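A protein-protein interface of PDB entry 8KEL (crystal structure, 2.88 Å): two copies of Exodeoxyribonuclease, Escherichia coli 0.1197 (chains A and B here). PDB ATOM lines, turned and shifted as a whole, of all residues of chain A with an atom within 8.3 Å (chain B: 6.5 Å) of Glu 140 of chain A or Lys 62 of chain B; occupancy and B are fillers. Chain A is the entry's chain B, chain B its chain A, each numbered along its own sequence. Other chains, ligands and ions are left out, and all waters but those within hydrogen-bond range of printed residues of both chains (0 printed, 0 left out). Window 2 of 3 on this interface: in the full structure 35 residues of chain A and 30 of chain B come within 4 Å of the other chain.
The side-chain carboxylate of Glu 140 of chain A is in salt-bridge range of the side-chain amino group of Lys 62 of chain B.
N of Lys 62 of chain B is in hydrogen-bond range of O of Asn 139 of chain A (2.8 Å).
Glu 138 of chain A touches Leu 59 of chain B (O to CD1, 3.8 Å).
Asn 139 of chain A touches Leu 59 of chain B (CA to CD1, 3.9 Å).
Asn 139 of chain A touches Phe 60 of chain B.
Thr 61 of chain B touches Asn 139 of chain A.
Ser 63 of chain B touches Asp 142 of chain A (OG to OD1, 3.99 Å).
Of the printed residues of chain B, Asn 139 of chain A touches Leu 59 (3.9 Å), Phe 60 (3.1 Å), Thr 61 (3.4 Å) and Lys 62 (2.8 Å).
Of the printed residues of chain B, Asp 142 of chain A touches Ser 63.
Of the printed residues of chain A, Leu 59 of chain B touches Glu 138 and Asn 139.
Of the printed residues of chain A, Phe 60 of chain B touches Asn 139 (3.1 Å).
Printed residues of chain A within 4 Å of Thr 61 of chain B: Asn 139.
Of chain A, only Asn 139 and Glu 140 come within 4 Å of Lys 62 of chain B.
Thr 64 of chain B touches none of the printed residues of chain A.
Trp 67 of chain B touches none of the printed residues of chain A.
The nearest residue of chain A that does not touch Lys 62 of chain B is Leu 141 of chain A (5.9 Å).
NH1 of Arg 128 of chain A is in salt-bridge range of OE2 of Glu 138 of chain A (3.9 Å).
The backbone carbonyl oxygen of Met 11 of chain B sits at hydrogen-bond distance from the backbone NH of Thr 61 of chain B (2.7 Å).
The side-chain amide nitrogen (NE2) of Gln 131 of chain A is in hydrogen-bond range of the backbone carbonyl oxygen (O) of Asp 142 of chain A (3.0 Å).
No position is printed for both chains.
Of the 7 pairs that touch across the chains among the printed residues, none has its exchanged pair printed and touching as well.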
ATOM      1  N   ARG A 128     -23.043  12.283   2.509  1.00  0.00           N
ATOM      2  CA  ARG A 128     -22.855  11.370   1.372  1.00  0.00           C
ATOM      3  C   ARG A 128     -23.939  10.314   1.259  1.00  0.00           C
ATOM      4  O   ARG A 128     -24.129   9.768   0.160  1.00  0.00           O
ATOM      5  CB  ARG A 128     -21.475  10.666   1.286  1.00  0.00           C
ATOM      6  CG  ARG A 128     -20.667  10.334   2.510  1.00  0.00           C
ATOM      7  CD  ARG A 128     -19.221  10.800   2.294  1.00  0.00           C
ATOM      8  NE  ARG A 128     -18.433  10.947   3.521  1.00  0.00           N
ATOM      9  CZ  ARG A 128     -17.869   9.976   4.246  1.00  0.00           C
ATOM     10  NH1 ARG A 128     -18.096   8.687   4.007  1.00  0.00           N
ATOM     11  NH2 ARG A 128     -17.110  10.309   5.287  1.00  0.00           N
ATOM     12  N   GLN A 131     -26.224  10.589  -1.516  1.00  0.00           N
ATOM     13  CA  GLN A 131     -25.651  10.101  -2.758  1.00  0.00           C
ATOM     14  C   GLN A 131     -25.551   8.593  -2.795  1.00  0.00           C
ATOM     15  O   GLN A 131     -25.801   7.989  -3.846  1.00  0.00           O
ATOM     16  CB  GLN A 131     -24.291  10.725  -2.984  1.00  0.00           C
ATOM     17  CG  GLN A 131     -24.374  12.080  -3.585  1.00  0.00           C
ATOM     18  CD  GLN A 131     -23.019  12.717  -3.654  1.00  0.00           C
ATOM     19  OE1 GLN A 131     -22.043  12.175  -3.132  1.00  0.00           O
ATOM     20  NE2 GLN A 131     -22.941  13.883  -4.288  1.00  0.00           N
ATOM     21  N   GLY A 135     -27.474   5.589  -5.588  1.00  0.00           N
ATOM     22  CA  GLY A 135     -26.719   4.566  -6.284  1.00  0.00           C
ATOM     23  C   GLY A 135     -25.274   4.916  -6.592  1.00  0.00           C
ATOM     24  O   GLY A 135     -24.584   4.113  -7.232  1.00  0.00           O
ATOM     25  N   VAL A 136     -24.796   6.084  -6.166  1.00  0.00           N
ATOM     26  CA  VAL A 136     -23.409   6.467  -6.383  1.00  0.00           C
ATOM     27  C   VAL A 136     -22.499   5.543  -5.576  1.00  0.00           C
ATOM     28  O   VAL A 136     -22.661   5.400  -4.354  1.00  0.00           O
ATOM     29  CB  VAL A 136     -23.201   7.939  -5.982  1.00  0.00           C
ATOM     30  CG1 VAL A 136     -21.761   8.359  -6.160  1.00  0.00           C
ATOM     31  CG2 VAL A 136     -24.132   8.834  -6.739  1.00  0.00           C
ATOM     32  N   SER A 137     -21.519   4.934  -6.253  1.00  0.00           N
ATOM     33  CA  SER A 137     -20.570   4.045  -5.594  1.00  0.00           C
ATOM     34  C   SER A 137     -19.654   4.819  -4.663  1.00  0.00           C
ATOM     35  O   SER A 137     -19.552   6.044  -4.725  1.00  0.00           O
ATOM     36  CB  SER A 137     -19.744   3.266  -6.609  1.00  0.00           C
ATOM     37  OG  SER A 137     -20.551   2.245  -7.177  1.00  0.00           O
ATOM     38  N   GLU A 138     -18.998   4.073  -3.768  1.00  0.00           N
ATOM     39  CA  GLU A 138     -18.307   4.687  -2.640  1.00  0.00           C
ATOM     40  C   GLU A 138     -17.041   5.425  -3.071  1.00  0.00           C
ATOM     41  O   GLU A 138     -16.616   6.347  -2.366  1.00  0.00           O
ATOM     42  CB  GLU A 138     -17.995   3.622  -1.576  1.00  0.00           C
ATOM     43  CG  GLU A 138     -17.436   4.152  -0.238  1.00  0.00           C
ATOM     44  CD  GLU A 138     -18.470   4.891   0.664  1.00  0.00           C
ATOM     45  OE1 GLU A 138     -19.693   4.612   0.568  1.00  0.00           O
ATOM     46  OE2 GLU A 138     -18.047   5.744   1.490  1.00  0.00           O
ATOM     47  N   ASN A 139     -16.423   5.036  -4.209  1.00  0.00           N
ATOM     48  CA  ASN A 139     -15.275   5.761  -4.772  1.00  0.00           C
ATOM     49  C   ASN A 139     -15.662   6.934  -5.655  1.00  0.00           C
ATOM     50  O   ASN A 139     -14.787   7.715  -6.041  1.00  0.00           O
ATOM     51  CB  ASN A 139     -14.376   4.859  -5.612  1.00  0.00           C
ATOM     52  CG  ASN A 139     -15.130   4.161  -6.671  1.00  0.00           C
ATOM     53  OD1 ASN A 139     -16.354   4.152  -6.643  1.00  0.00           O
ATOM     54  ND2 ASN A 139     -14.429   3.646  -7.673  1.00  0.00           N
ATOM     55  N   GLU A 140     -16.933   7.069  -5.997  1.00  0.00           N
ATOM     56  CA  GLU A 140     -17.388   8.134  -6.870  1.00  0.00           C
ATOM     57  C   GLU A 140     -18.245   9.153  -6.140  1.00  0.00           C
ATOM     58  O   GLU A 140     -18.842  10.013  -6.783  1.00  0.00           O
ATOM     59  CB  GLU A 140     -18.096   7.512  -8.062  1.00  0.00           C
ATOM     60  CG  GLU A 140     -17.066   6.888  -8.970  1.00  0.00           C
ATOM     61  CD  GLU A 140     -17.619   5.985 -10.063  1.00  0.00           C
ATOM     62  OE1 GLU A 140     -18.786   5.525  -9.955  1.00  0.00           O
ATOM     63  OE2 GLU A 140     -16.873   5.764 -11.059  1.00  0.00           O
ATOM     64  N   LEU A 141     -18.279   9.106  -4.814  1.00  0.00           N
ATOM     65  CA  LEU A 141     -18.959  10.129  -4.035  1.00  0.00           C
ATOM     66  C   LEU A 141     -18.221  11.456  -4.182  1.00  0.00           C
ATOM     67  O   LEU A 141     -16.990  11.492  -4.244  1.00  0.00           O
ATOM     68  CB  LEU A 141     -19.030   9.723  -2.544  1.00  0.00           C
ATOM     69  CG  LEU A 141     -19.738   8.425  -2.043  1.00  0.00           C
ATOM     70  CD1 LEU A 141     -19.535   8.193  -0.562  1.00  0.00           C
ATOM     71  CD2 LEU A 141     -21.245   8.316  -2.391  1.00  0.00           C
ATOM     72  N   ASP A 142     -18.971  12.552  -4.255  1.00  0.00           N
ATOM     73  CA  ASP A 142     -18.363  13.879  -4.216  1.00  0.00           C
ATOM     74  C   ASP A 142     -19.312  14.884  -3.597  1.00  0.00           C
ATOM     75  O   ASP A 142     -20.262  15.316  -4.246  1.00  0.00           O
ATOM     76  CB  ASP A 142     -17.961  14.370  -5.587  1.00  0.00           C
ATOM     77  CG  ASP A 142     -17.327  15.713  -5.494  1.00  0.00           C
ATOM     78  OD1 ASP A 142     -16.190  15.755  -4.990  1.00  0.00           O
ATOM     79  OD2 ASP A 142     -17.976  16.721  -5.831  1.00  0.00           O
ATOM     80  N   THR A 143     -19.007  15.323  -2.389  1.00  0.00           N
ATOM     81  CA  THR A 143     -19.878  16.222  -1.656  1.00  0.00           C
ATOM     82  C   THR A 143     -19.287  17.614  -1.546  1.00  0.00           C
ATOM     83  O   THR A 143     -19.686  18.370  -0.662  1.00  0.00           O
ATOM     84  CB  THR A 143     -20.182  15.674  -0.252  1.00  0.00           C
ATOM     85  OG1 THR A 143     -18.975  15.605   0.517  1.00  0.00           O
ATOM     86  CG2 THR A 143     -20.843  14.271  -0.302  1.00  0.00           C
ATOM     87  N   MET B  11      -5.182   9.065  -1.544  1.00  0.00           N
ATOM     88  CA  MET B  11      -5.978   8.860  -2.753  1.00  0.00           C
ATOM     89  C   MET B  11      -7.490   8.911  -2.524  1.00  0.00           C
ATOM     90  O   MET B  11      -8.251   8.484  -3.403  1.00  0.00           O
ATOM     91  CB  MET B  11      -5.646   7.515  -3.381  1.00  0.00           C
ATOM     92  CG  MET B  11      -4.339   7.491  -4.048  1.00  0.00           C
ATOM     93  SD  MET B  11      -4.329   8.644  -5.435  1.00  0.00           S
ATOM     94  CE  MET B  11      -2.585   8.579  -5.796  1.00  0.00           C
ATOM     95  N   LEU B  59      -9.784   3.295   0.401  1.00  0.00           N
ATOM     96  CA  LEU B  59     -10.682   3.904  -0.570  1.00  0.00           C
ATOM     97  C   LEU B  59      -9.931   4.797  -1.559  1.00  0.00           C
ATOM     98  O   LEU B  59      -9.306   5.786  -1.159  1.00  0.00           O
ATOM     99  CB  LEU B  59     -11.752   4.699   0.176  1.00  0.00           C
ATOM    100  CG  LEU B  59     -12.790   5.360  -0.720  1.00  0.00           C
ATOM    101  CD1 LEU B  59     -13.509   4.306  -1.575  1.00  0.00           C
ATOM    102  CD2 LEU B  59     -13.742   6.165   0.146  1.00  0.00           C
ATOM    103  N   PHE B  60     -10.030   4.489  -2.859  1.00  0.00           N
ATOM    104  CA  PHE B  60      -9.454   5.365  -3.876  1.00  0.00           C
ATOM    105  C   PHE B  60     -10.582   6.163  -4.537  1.00  0.00           C
ATOM    106  O   PHE B  60     -11.332   5.628  -5.362  1.00  0.00           O
ATOM    107  CB  PHE B  60      -8.633   4.634  -4.944  1.00  0.00           C
ATOM    108  CG  PHE B  60      -7.520   3.757  -4.415  1.00  0.00           C
ATOM    109  CD1 PHE B  60      -7.701   2.899  -3.351  1.00  0.00           C
ATOM    110  CD2 PHE B  60      -6.227   3.982  -4.842  1.00  0.00           C
ATOM    111  CE1 PHE B  60      -6.662   2.128  -2.865  1.00  0.00           C
ATOM    112  CE2 PHE B  60      -5.168   3.250  -4.324  1.00  0.00           C
ATOM    113  CZ  PHE B  60      -5.396   2.318  -3.332  1.00  0.00           C
ATOM    114  N   THR B  61     -10.667   7.447  -4.199  1.00  0.00           N
ATOM    115  CA  THR B  61     -11.735   8.336  -4.633  1.00  0.00           C
ATOM    116  C   THR B  61     -11.401   8.920  -5.993  1.00  0.00           C
ATOM    117  O   THR B  61     -10.281   9.378  -6.207  1.00  0.00           O
ATOM    118  CB  THR B  61     -11.886   9.475  -3.635  1.00  0.00           C
ATOM    119  OG1 THR B  61     -12.026   8.919  -2.328  1.00  0.00           O
ATOM    120  CG2 THR B  61     -13.089  10.334  -3.960  1.00  0.00           C
ATOM    121  N   LYS B  62     -12.385   8.946  -6.893  1.00  0.00           N
ATOM    122  CA  LYS B  62     -12.139   9.412  -8.256  1.00  0.00           C
ATOM    123  C   LYS B  62     -11.764  10.894  -8.324  1.00  0.00           C
ATOM    124  O   LYS B  62     -10.926  11.276  -9.144  1.00  0.00           O
ATOM    125  CB  LYS B  62     -13.352   9.134  -9.131  1.00  0.00           C
ATOM    126  CG  LYS B  62     -13.215   7.886  -9.991  1.00  0.00           C
ATOM    127  CD  LYS B  62     -12.991   6.649  -9.143  1.00  0.00           C
ATOM    128  CE  LYS B  62     -12.798   5.399 -10.004  1.00  0.00           C
ATOM    129  NZ  LYS B  62     -14.030   5.052 -10.778  1.00  0.00           N
ATOM    130  N   SER B  63     -12.384  11.757  -7.514  1.00  0.00           N
ATOM    131  CA  SER B  63     -12.010  13.167  -7.575  1.00  0.00           C
ATOM    132  C   SER B  63     -10.556  13.366  -7.170  1.00  0.00           C
ATOM    133  O   SER B  63      -9.834  14.156  -7.790  1.00  0.00           O
ATOM    134  CB  SER B  63     -12.927  14.024  -6.698  1.00  0.00           C
ATOM    135  OG  SER B  63     -12.691  13.855  -5.313  1.00  0.00           O
ATOM    136  N   THR B  64     -10.107  12.655  -6.132  1.00  0.00           N
ATOM    137  CA  THR B  64      -8.715  12.754  -5.696  1.00  0.00           C
ATOM    138  C   THR B  64      -7.766  12.145  -6.724  1.00  0.00           C
ATOM    139  O   THR B  64      -6.650  12.637  -6.912  1.00  0.00           O
ATOM    140  CB  THR B  64      -8.550  12.072  -4.342  1.00  0.00           C
ATOM    141  OG1 THR B  64      -9.462  12.659  -3.409  1.00  0.00           O
ATOM    142  CG2 THR B  64      -7.138  12.260  -3.816  1.00  0.00           C
ATOM    143  N   ILE B  65      -8.179  11.069  -7.388  1.00  0.00           N
ATOM    144  CA  ILE B  65      -7.348  10.512  -8.446  1.00  0.00           C
ATOM    145  C   ILE B  65      -7.237  11.484  -9.619  1.00  0.00           C
ATOM    146  O   ILE B  65      -6.164  11.645 -10.208  1.00  0.00           O
ATOM    147  CB  ILE B  65      -7.880   9.135  -8.873  1.00  0.00           C
ATOM    148  CG1 ILE B  65      -7.650   8.140  -7.733  1.00  0.00           C
ATOM    149  CG2 ILE B  65      -7.217   8.658 -10.152  1.00  0.00           C
ATOM    150  CD1 ILE B  65      -8.265   6.787  -7.968  1.00  0.00           C
ATOM    151  N   GLU B  66      -8.337  12.156  -9.975  1.00  0.00           N
ATOM    152  CA  GLU B  66      -8.255  13.197 -10.997  1.00  0.00           C
ATOM    153  C   GLU B  66      -7.322  14.318 -10.556  1.00  0.00           C
ATOM    154  O   GLU B  66      -6.479  14.773 -11.332  1.00  0.00           O
ATOM    155  CB  GLU B  66      -9.660  13.735 -11.325  1.00  0.00           C
ATOM    156  CG  GLU B  66     -10.481  12.815 -12.270  1.00  0.00           C
ATOM    157  CD  GLU B  66     -11.952  13.247 -12.479  1.00  0.00           C
ATOM    158  OE1 GLU B  66     -12.441  14.134 -11.740  1.00  0.00           O
ATOM    159  OE2 GLU B  66     -12.618  12.695 -13.396  1.00  0.00           O
ATOM    160  N   TRP B  67      -7.429  14.738  -9.301  1.00  0.00           N
ATOM    161  CA  TRP B  67      -6.629  15.849  -8.798  1.00  0.00           C
ATOM    162  C   TRP B  67      -5.124  15.583  -8.929  1.00  0.00           C
ATOM    163  O   TRP B  67      -4.352  16.499  -9.232  1.00  0.00           O
ATOM    164  CB  TRP B  67      -7.008  16.082  -7.343  1.00  0.00           C
ATOM    165  CG  TRP B  67      -6.291  17.177  -6.670  1.00  0.00           C
ATOM    166  CD1 TRP B  67      -6.641  18.483  -6.630  1.00  0.00           C
ATOM    167  CD2 TRP B  67      -5.036  17.073  -5.991  1.00  0.00           C
ATOM    168  NE1 TRP B  67      -5.717  19.198  -5.910  1.00  0.00           N
ATOM    169  CE2 TRP B  67      -4.709  18.358  -5.522  1.00  0.00           C
ATOM    170  CE3 TRP B  67      -4.168  16.010  -5.715  1.00  0.00           C
ATOM    171  CZ2 TRP B  67      -3.549  18.615  -4.790  1.00  0.00           C
ATOM    172  CZ3 TRP B  67      -3.019  16.266  -4.989  1.00  0.00           C
ATOM    173  CH2 TRP B  67      -2.719  17.560  -4.535  1.00  0.00           C
